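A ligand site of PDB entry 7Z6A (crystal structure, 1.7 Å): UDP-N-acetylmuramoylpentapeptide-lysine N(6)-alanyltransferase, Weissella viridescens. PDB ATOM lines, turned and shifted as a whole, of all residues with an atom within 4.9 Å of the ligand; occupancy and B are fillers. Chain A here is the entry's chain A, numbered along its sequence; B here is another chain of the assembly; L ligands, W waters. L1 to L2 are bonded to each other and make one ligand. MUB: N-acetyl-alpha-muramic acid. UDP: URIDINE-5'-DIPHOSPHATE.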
ATOM      1  N   LYS A  37       0.542  23.124   4.840  1.00  0.00           N
ATOM      2  CA  LYS A  37       0.506  22.898   3.377  1.00  0.00           C
ATOM      3  C   LYS A  37       1.062  24.149   2.687  1.00  0.00           C
ATOM      4  O   LYS A  37       0.360  24.735   1.878  1.00  0.00           O
ATOM      5  CB  LYS A  37      -0.934  22.619   2.968  1.00  0.00           C
ATOM      6  CG  LYS A  37      -1.566  21.416   3.639  1.00  0.00           C
ATOM      7  CD  LYS A  37      -1.041  20.085   3.154  1.00  0.00           C
ATOM      8  CE  LYS A  37      -1.852  18.901   3.651  1.00  0.00           C
ATOM      9  NZ  LYS A  37      -1.114  17.625   3.529  1.00  0.00           N
ATOM     10  N   ASN A  39       3.012  24.520   0.340  1.00  0.00           N
ATOM     11  CA  ASN A  39       3.155  24.441  -1.115  1.00  0.00           C
ATOM     12  C   ASN A  39       1.821  24.568  -1.845  1.00  0.00           C
ATOM     13  O   ASN A  39       1.778  24.452  -3.080  1.00  0.00           O
ATOM     14  CB  ASN A  39       3.826  23.122  -1.499  1.00  0.00           C
ATOM     15  CG  ASN A  39       3.209  21.893  -0.830  1.00  0.00           C
ATOM     16  OD1 ASN A  39       2.735  21.961   0.321  1.00  0.00           O
ATOM     17  ND2 ASN A  39       3.245  20.754  -1.519  1.00  0.00           N
ATOM     18  N   TRP A  40       0.742  24.831  -1.116  1.00  0.00           N
ATOM     19  CA  TRP A  40      -0.583  25.080  -1.678  1.00  0.00           C
ATOM     20  C   TRP A  40      -0.964  26.536  -1.460  1.00  0.00           C
ATOM     21  O   TRP A  40      -0.444  27.213  -0.572  1.00  0.00           O
ATOM     22  CB  TRP A  40      -1.627  24.163  -1.016  1.00  0.00           C
ATOM     23  CG  TRP A  40      -1.427  22.674  -1.244  1.00  0.00           C
ATOM     24  CD1 TRP A  40      -0.359  21.908  -0.828  1.00  0.00           C
ATOM     25  CD2 TRP A  40      -2.334  21.780  -1.890  1.00  0.00           C
ATOM     26  NE1 TRP A  40      -0.544  20.600  -1.215  1.00  0.00           N
ATOM     27  CE2 TRP A  40      -1.755  20.487  -1.850  1.00  0.00           C
ATOM     28  CE3 TRP A  40      -3.598  21.928  -2.479  1.00  0.00           C
ATOM     29  CZ2 TRP A  40      -2.383  19.374  -2.397  1.00  0.00           C
ATOM     30  CZ3 TRP A  40      -4.205  20.824  -3.034  1.00  0.00           C
ATOM     31  CH2 TRP A  40      -3.610  19.561  -2.991  1.00  0.00           C
ATOM     32  N   ASP A  64      -1.384  22.305  -7.814  1.00  0.00           N
ATOM     33  CA  ASP A  64      -1.066  22.199  -9.221  1.00  0.00           C
ATOM     34  C   ASP A  64      -1.532  20.854  -9.782  1.00  0.00           C
ATOM     35  O   ASP A  64      -1.702  19.875  -9.065  1.00  0.00           O
ATOM     36  CB  ASP A  64       0.441  22.375  -9.426  1.00  0.00           C
ATOM     37  CG  ASP A  64       0.862  23.828  -9.343  1.00  0.00           C
ATOM     38  OD1 ASP A  64       0.136  24.696  -9.876  1.00  0.00           O
ATOM     39  OD2 ASP A  64       1.924  24.100  -8.739  1.00  0.00           O
ATOM     40  N   THR A  65      -1.770  20.835 -11.087  1.00  0.00           N
ATOM     41  CA  THR A  65      -2.149  19.645 -11.855  1.00  0.00           C
ATOM     42  C   THR A  65      -1.342  19.647 -13.148  1.00  0.00           C
ATOM     43  O   THR A  65      -0.682  20.651 -13.448  1.00  0.00           O
ATOM     44  CB  THR A  65      -3.638  19.648 -12.218  1.00  0.00           C
ATOM     45  OG1 THR A  65      -3.852  20.531 -13.322  1.00  0.00           O
ATOM     46  CG2 THR A  65      -4.519  20.058 -11.028  1.00  0.00           C
ATOM     47  N   PHE A  71      -6.298  22.522  -8.672  1.00  0.00           N
ATOM     48  CA  PHE A  71      -7.194  21.675  -7.894  1.00  0.00           C
ATOM     49  C   PHE A  71      -7.487  22.404  -6.582  1.00  0.00           C
ATOM     50  O   PHE A  71      -6.569  22.688  -5.814  1.00  0.00           O
ATOM     51  CB  PHE A  71      -6.512  20.323  -7.652  1.00  0.00           C
ATOM     52  CG  PHE A  71      -7.211  19.411  -6.656  1.00  0.00           C
ATOM     53  CD1 PHE A  71      -8.476  18.923  -6.914  1.00  0.00           C
ATOM     54  CD2 PHE A  71      -6.553  19.004  -5.507  1.00  0.00           C
ATOM     55  CE1 PHE A  71      -9.097  18.062  -6.017  1.00  0.00           C
ATOM     56  CE2 PHE A  71      -7.154  18.140  -4.613  1.00  0.00           C
ATOM     57  CZ  PHE A  71      -8.444  17.674  -4.859  1.00  0.00           C
ATOM     58  N   TYR A 104     -10.357  23.588 -11.709  1.00  0.00           N
ATOM     59  CA  TYR A 104     -11.268  22.749 -12.473  1.00  0.00           C
ATOM     60  C   TYR A 104     -12.337  22.098 -11.620  1.00  0.00           C
ATOM     61  O   TYR A 104     -13.360  21.650 -12.153  1.00  0.00           O
ATOM     62  CB  TYR A 104     -10.473  21.672 -13.222  1.00  0.00           C
ATOM     63  CG  TYR A 104      -9.986  20.482 -12.413  1.00  0.00           C
ATOM     64  CD1 TYR A 104      -8.746  20.517 -11.770  1.00  0.00           C
ATOM     65  CD2 TYR A 104     -10.729  19.307 -12.334  1.00  0.00           C
ATOM     66  CE1 TYR A 104      -8.283  19.411 -11.032  1.00  0.00           C
ATOM     67  CE2 TYR A 104     -10.278  18.193 -11.598  1.00  0.00           C
ATOM     68  CZ  TYR A 104      -9.044  18.256 -10.965  1.00  0.00           C
ATOM     69  OH  TYR A 104      -8.604  17.157 -10.255  1.00  0.00           O
ATOM     70  N   ARG A 107     -13.260  20.403  -4.367  1.00  0.00           N
ATOM     71  CA  ARG A 107     -13.570  19.160  -3.669  1.00  0.00           C
ATOM     72  C   ARG A 107     -13.596  19.416  -2.168  1.00  0.00           C
ATOM     73  O   ARG A 107     -12.725  20.112  -1.636  1.00  0.00           O
ATOM     74  CB  ARG A 107     -12.521  18.089  -3.970  1.00  0.00           C
ATOM     75  CG  ARG A 107     -12.729  16.783  -3.184  1.00  0.00           C
ATOM     76  CD  ARG A 107     -11.828  15.685  -3.769  1.00  0.00           C
ATOM     77  NE  ARG A 107     -12.275  15.293  -5.088  1.00  0.00           N
ATOM     78  CZ  ARG A 107     -11.552  14.564  -5.926  1.00  0.00           C
ATOM     79  NH1 ARG A 107     -10.345  14.130  -5.590  1.00  0.00           N
ATOM     80  NH2 ARG A 107     -12.038  14.287  -7.135  1.00  0.00           N
ATOM     81  N   ILE A 143      -8.975  10.963  -1.094  1.00  0.00           N
ATOM     82  CA  ILE A 143      -7.763  11.519  -0.494  1.00  0.00           C
ATOM     83  C   ILE A 143      -7.684  11.157   0.981  1.00  0.00           C
ATOM     84  O   ILE A 143      -6.688  10.600   1.442  1.00  0.00           O
ATOM     85  CB  ILE A 143      -7.690  13.041  -0.711  1.00  0.00           C
ATOM     86  CG1 ILE A 143      -7.658  13.360  -2.219  1.00  0.00           C
ATOM     87  CG2 ILE A 143      -6.467  13.632   0.027  1.00  0.00           C
ATOM     88  CD1 ILE A 143      -8.009  14.812  -2.567  1.00  0.00           C
ATOM     89  N   THR A 210       7.346   5.829   1.654  1.00  0.00           N
ATOM     90  CA  THR A 210       7.734   7.223   1.710  1.00  0.00           C
ATOM     91  C   THR A 210       7.189   7.883   2.974  1.00  0.00           C
ATOM     92  O   THR A 210       6.139   7.489   3.505  1.00  0.00           O
ATOM     93  CB  THR A 210       7.211   7.948   0.463  1.00  0.00           C
ATOM     94  OG1 THR A 210       7.509   9.336   0.552  1.00  0.00           O
ATOM     95  CG2 THR A 210       5.701   7.741   0.322  1.00  0.00           C
ATOM     96  N   HIS A 211       7.914   8.875   3.472  1.00  0.00           N
ATOM     97  CA  HIS A 211       7.519   9.630   4.655  1.00  0.00           C
ATOM     98  C   HIS A 211       7.596  11.116   4.343  1.00  0.00           C
ATOM     99  O   HIS A 211       8.303  11.544   3.418  1.00  0.00           O
ATOM    100  CB  HIS A 211       8.397   9.262   5.882  1.00  0.00           C
ATOM    101  CG  HIS A 211       9.849   9.579   5.689  1.00  0.00           C
ATOM    102  ND1 HIS A 211      10.400  10.785   6.050  1.00  0.00           N
ATOM    103  CD2 HIS A 211      10.860   8.838   5.179  1.00  0.00           C
ATOM    104  CE1 HIS A 211      11.694  10.776   5.764  1.00  0.00           C
ATOM    105  NE2 HIS A 211      11.997   9.607   5.230  1.00  0.00           N
ATOM    106  N   ARG A 212       6.858  11.912   5.114  1.00  0.00           N
ATOM    107  CA  ARG A 212       6.885  13.354   4.971  1.00  0.00           C
ATOM    108  C   ARG A 212       8.171  13.921   5.585  1.00  0.00           C
ATOM    109  O   ARG A 212       8.703  13.369   6.548  1.00  0.00           O
ATOM    110  CB  ARG A 212       5.675  13.959   5.654  1.00  0.00           C
ATOM    111  CG  ARG A 212       4.381  13.538   5.021  1.00  0.00           C
ATOM    112  CD  ARG A 212       3.251  14.414   5.541  1.00  0.00           C
ATOM    113  NE  ARG A 212       1.946  14.019   5.052  1.00  0.00           N
ATOM    114  CZ  ARG A 212       1.394  14.532   3.961  1.00  0.00           C
ATOM    115  NH1 ARG A 212       2.028  15.424   3.234  1.00  0.00           N
ATOM    116  NH2 ARG A 212       0.172  14.132   3.589  1.00  0.00           N
ATOM    117  N   PRO A 213       8.665  15.048   5.071  1.00  0.00           N
ATOM    118  CA  PRO A 213       9.864  15.664   5.644  1.00  0.00           C
ATOM    119  C   PRO A 213       9.571  16.223   7.031  1.00  0.00           C
ATOM    120  O   PRO A 213       8.416  16.542   7.358  1.00  0.00           O
ATOM    121  CB  PRO A 213      10.222  16.783   4.655  1.00  0.00           C
ATOM    122  CG  PRO A 213       9.279  16.652   3.517  1.00  0.00           C
ATOM    123  CD  PRO A 213       8.125  15.835   3.942  1.00  0.00           C
ATOM    124  N   TYR A 216       7.567  19.424   7.584  1.00  0.00           N
ATOM    125  CA  TYR A 216       6.098  19.369   7.579  1.00  0.00           C
ATOM    126  C   TYR A 216       5.555  19.463   8.998  1.00  0.00           C
ATOM    127  O   TYR A 216       4.617  20.230   9.297  1.00  0.00           O
ATOM    128  CB  TYR A 216       5.659  18.070   6.906  1.00  0.00           C
ATOM    129  CG  TYR A 216       4.157  17.882   6.719  1.00  0.00           C
ATOM    130  CD1 TYR A 216       3.385  17.235   7.665  1.00  0.00           C
ATOM    131  CD2 TYR A 216       3.523  18.325   5.553  1.00  0.00           C
ATOM    132  CE1 TYR A 216       1.995  17.047   7.474  1.00  0.00           C
ATOM    133  CE2 TYR A 216       2.163  18.136   5.350  1.00  0.00           C
ATOM    134  CZ  TYR A 216       1.392  17.493   6.309  1.00  0.00           C
ATOM    135  OH  TYR A 216       0.030  17.326   6.061  1.00  0.00           O
ATOM    136  N   LEU A 333      -8.900  14.127 -15.399  1.00  0.00           N
ATOM    137  CA  LEU A 333      -8.122  13.843 -14.186  1.00  0.00           C
ATOM    138  C   LEU A 333      -8.837  12.952 -13.179  1.00  0.00           C
ATOM    139  O   LEU A 333      -8.171  12.327 -12.364  1.00  0.00           O
ATOM    140  CB  LEU A 333      -7.681  15.152 -13.508  1.00  0.00           C
ATOM    141  CG  LEU A 333      -6.820  16.149 -14.282  1.00  0.00           C
ATOM    142  CD1 LEU A 333      -6.552  17.441 -13.486  1.00  0.00           C
ATOM    143  CD2 LEU A 333      -5.474  15.527 -14.723  1.00  0.00           C
ATOM    144  N   ALA B   1       1.577   9.698   1.350  1.00  0.00           N
ATOM    145  CA  ALA B   1       0.868   8.663   0.598  1.00  0.00           C
ATOM    146  C   ALA B   1      -0.643   8.777   0.785  1.00  0.00           C
ATOM    147  O   ALA B   1      -1.092   9.321   1.793  1.00  0.00           O
ATOM    148  CB  ALA B   1       1.354   7.291   1.024  1.00  0.00           C
ATOM    149  N   FGA B   2      -1.354   8.282  -0.089  1.00  0.00           N
ATOM    150  CA  FGA B   2      -2.807   8.094  -0.200  1.00  0.00           C
ATOM    151  C   FGA B   2      -3.480   8.443  -1.486  1.00  0.00           C
ATOM    152  O   FGA B   2      -4.721   8.991  -1.469  1.00  0.00           O
ATOM    153  CB  FGA B   2      -3.172   6.576   0.049  1.00  0.00           C
ATOM    154  CG  FGA B   2      -3.120   6.198   1.572  1.00  0.00           C
ATOM    155  CD  FGA B   2      -3.891   6.892   2.483  1.00  0.00           C
ATOM    156  OE1 FGA B   2      -5.156   7.310   2.308  1.00  0.00           O
ATOM    157  OXT FGA B   2      -2.901   8.296  -2.588  1.00  0.00           O
ATOM    158  N   DAL B   4      -3.664  10.156   3.652  1.00  0.00           N
ATOM    159  CA  DAL B   4      -3.893  11.604   3.497  1.00  0.00           C
ATOM    160  CB  DAL B   4      -3.441  12.085   2.118  1.00  0.00           C
ATOM    161  C   DAL B   4      -3.203  12.425   4.601  1.00  0.00           C
ATOM    162  O   DAL B   4      -1.981  12.354   4.775  1.00  0.00           O
ATOM    163  N   DAL B   5      -3.987  13.218   5.327  1.00  0.00           N
ATOM    164  CA  DAL B   5      -3.481  14.029   6.443  1.00  0.00           C
ATOM    165  CB  DAL B   5      -4.655  14.777   7.138  1.00  0.00           C
ATOM    166  C   DAL B   5      -2.385  15.028   6.040  1.00  0.00           C
ATOM    167  O   DAL B   5      -1.355  15.173   6.740  1.00  0.00           O
ATOM    168  OXT DAL B   5      -2.488  15.687   5.004  1.00  0.00           O
HETATM  169  C1  MUB L   1       2.262  15.535  -1.228  1.00  0.00           C
HETATM  170  C2  MUB L   1       2.456  14.051  -0.957  1.00  0.00           C
HETATM  171  C3  MUB L   1       3.503  13.864   0.139  1.00  0.00           C
HETATM  172  C4  MUB L   1       4.757  14.654  -0.179  1.00  0.00           C
HETATM  173  C5  MUB L   1       4.425  16.115  -0.457  1.00  0.00           C
HETATM  174  C6  MUB L   1       5.631  16.927  -0.874  1.00  0.00           C
HETATM  175  C7  MUB L   1       0.678  12.433  -1.342  1.00  0.00           C
HETATM  176  C8  MUB L   1      -0.650  11.908  -0.908  1.00  0.00           C
HETATM  177  C9  MUB L   1       3.413  11.737   1.333  1.00  0.00           C
HETATM  178  C10 MUB L   1       2.672  10.487   0.891  1.00  0.00           C
HETATM  179  C11 MUB L   1       4.641  11.367   2.129  1.00  0.00           C
HETATM  180  O1  MUB L   1       1.808  16.126  -0.054  1.00  0.00           O
HETATM  181  O3  MUB L   1       3.830  12.472   0.174  1.00  0.00           O
HETATM  182  O4  MUB L   1       5.689  14.576   0.906  1.00  0.00           O
HETATM  183  O5  MUB L   1       3.485  16.157  -1.558  1.00  0.00           O
HETATM  184  O6  MUB L   1       6.120  16.476  -2.127  1.00  0.00           O
HETATM  185  O7  MUB L   1       1.270  11.988  -2.319  1.00  0.00           O
HETATM  186  O10 MUB L   1       2.922  10.066  -0.263  1.00  0.00           O
HETATM  187  N2  MUB L   1       1.192  13.418  -0.609  1.00  0.00           N
HETATM  188  N1  UDP L   2      -5.104  15.398  -5.936  1.00  0.00           N
HETATM  189  C2  UDP L   2      -6.311  15.113  -6.541  1.00  0.00           C
HETATM  190  N3  UDP L   2      -6.592  15.862  -7.662  1.00  0.00           N
HETATM  191  C4  UDP L   2      -5.800  16.852  -8.216  1.00  0.00           C
HETATM  192  C5  UDP L   2      -4.561  17.089  -7.523  1.00  0.00           C
HETATM  193  C6  UDP L   2      -4.257  16.368  -6.423  1.00  0.00           C
HETATM  194  O2  UDP L   2      -7.077  14.250  -6.128  1.00  0.00           O
HETATM  195  O4  UDP L   2      -6.176  17.448  -9.229  1.00  0.00           O
HETATM  196  C1' UDP L   2      -4.720  14.616  -4.744  1.00  0.00           C
HETATM  197  C2' UDP L   2      -3.376  13.910  -4.883  1.00  0.00           C
HETATM  198  O2' UDP L   2      -3.572  12.699  -5.621  1.00  0.00           O
HETATM  199  C3' UDP L   2      -3.035  13.646  -3.404  1.00  0.00           C
HETATM  200  C4' UDP L   2      -3.737  14.807  -2.685  1.00  0.00           C
HETATM  201  O4' UDP L   2      -4.533  15.492  -3.666  1.00  0.00           O
HETATM  202  O3' UDP L   2      -3.611  12.426  -2.942  1.00  0.00           O
HETATM  203  C5' UDP L   2      -2.812  15.785  -2.011  1.00  0.00           C
HETATM  204  O5' UDP L   2      -2.205  15.104  -0.901  1.00  0.00           O
HETATM  205  PA  UDP L   2      -1.550  15.910   0.275  1.00  0.00           P
HETATM  206  O1A UDP L   2      -2.644  16.667   0.938  1.00  0.00           O
HETATM  207  O2A UDP L   2      -0.743  14.975   1.183  1.00  0.00           O
HETATM  208  O3A UDP L   2      -0.520  16.900  -0.441  1.00  0.00           O
HETATM  209  PB  UDP L   2       0.896  17.391   0.079  1.00  0.00           P
HETATM  210  O1B UDP L   2       0.849  17.896   1.466  1.00  0.00           O
HETATM  211  O3B UDP L   2       1.309  18.440  -0.955  1.00  0.00           O
HETATM  212  O   HOH W   1      -4.237  15.879   3.091  1.00  0.00           O
HETATM  213  O   HOH W   2       4.795  16.409   3.204  1.00  0.00           O
HETATM  214  O   HOH W   3      -3.787  19.032   0.500  1.00  0.00           O
HETATM  215  O   HOH W   4       2.622  19.818   2.170  1.00  0.00           O
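An oxygen (O4) of UDP L2 is in hydrogen-bond range of the side-chain hydroxyl (OH) of Tyr 104. NZ of Lys 37 is in salt-bridge range of O1B of UDP L2 (2.9 Å). The side-chain amide nitrogen (ND2) of Asn 39 is in hydrogen-bond range of an oxygen (O3B) of UDP L2, at 3.1 Å. The guanidinium group (NH2) of Arg 212 is in salt-bridge range of an oxygen (O2A) of UDP L2, at 2.7 Å. C10 of MUB L1 is bonded to N of Ala 1 of chain B. NE1 of Trp 40 is in hydrogen-bond range of O3B of UDP L2 (2.9 Å). The guanidinium group of Arg 107 is in hydrogen-bond range of an oxygen (O2) of UDP L2, 3.3 Å away.
The side-chain hydroxyl (OH) of Tyr 216 sits at hydrogen-bond distance from the side-chain amino group (NZ) of Lys 37 (2.8 Å). The guanidinium group (NH2) of Arg 212 lies within salt-bridge range of OXT of DAL 5 of chain B. OXT of DAL 5 of chain B is in salt-bridge range of the side-chain amino group (NZ) of Lys 37 (2.8 Å). OE1 of FGA 2 of chain B lies close to N of DAL 4 of chain B (3.5 Å). NH2 of Arg 212 is in hydrogen-bond range of O of DAL 4 of chain B (3.0 Å).
Residues that only touch the ligand: Thr 65, Phe 71, Ile 143, Thr 210, His 211 and FGA 2 of chain B. Hydrophobic or aromatic side chains that line the ligand: Trp 40, Phe 71, Tyr 104, Ile 143 and Ala 1 of chain B. 13 residues have an atom within 4 Å of the ligand: Lys 37, Asn 39, Trp 40, Thr 65, Phe 71, Tyr 104, Arg 107, Ile 143, Thr 210, His 211, Arg 212, Ala 1 of chain B and FGA 2 of chain B.
Water W4 bridges O1B of UDP L2 (2.7 Å) and OD1 of Asn 39 (2.8 Å). Water W1 lies within hydrogen-bond range of OXT of DAL 5 of chain B (2.6 Å) and an oxygen (O1A) of UDP L2 (2.8 Å). Water W2 bridges NH1 of Arg 212 and O4 of MUB L1.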
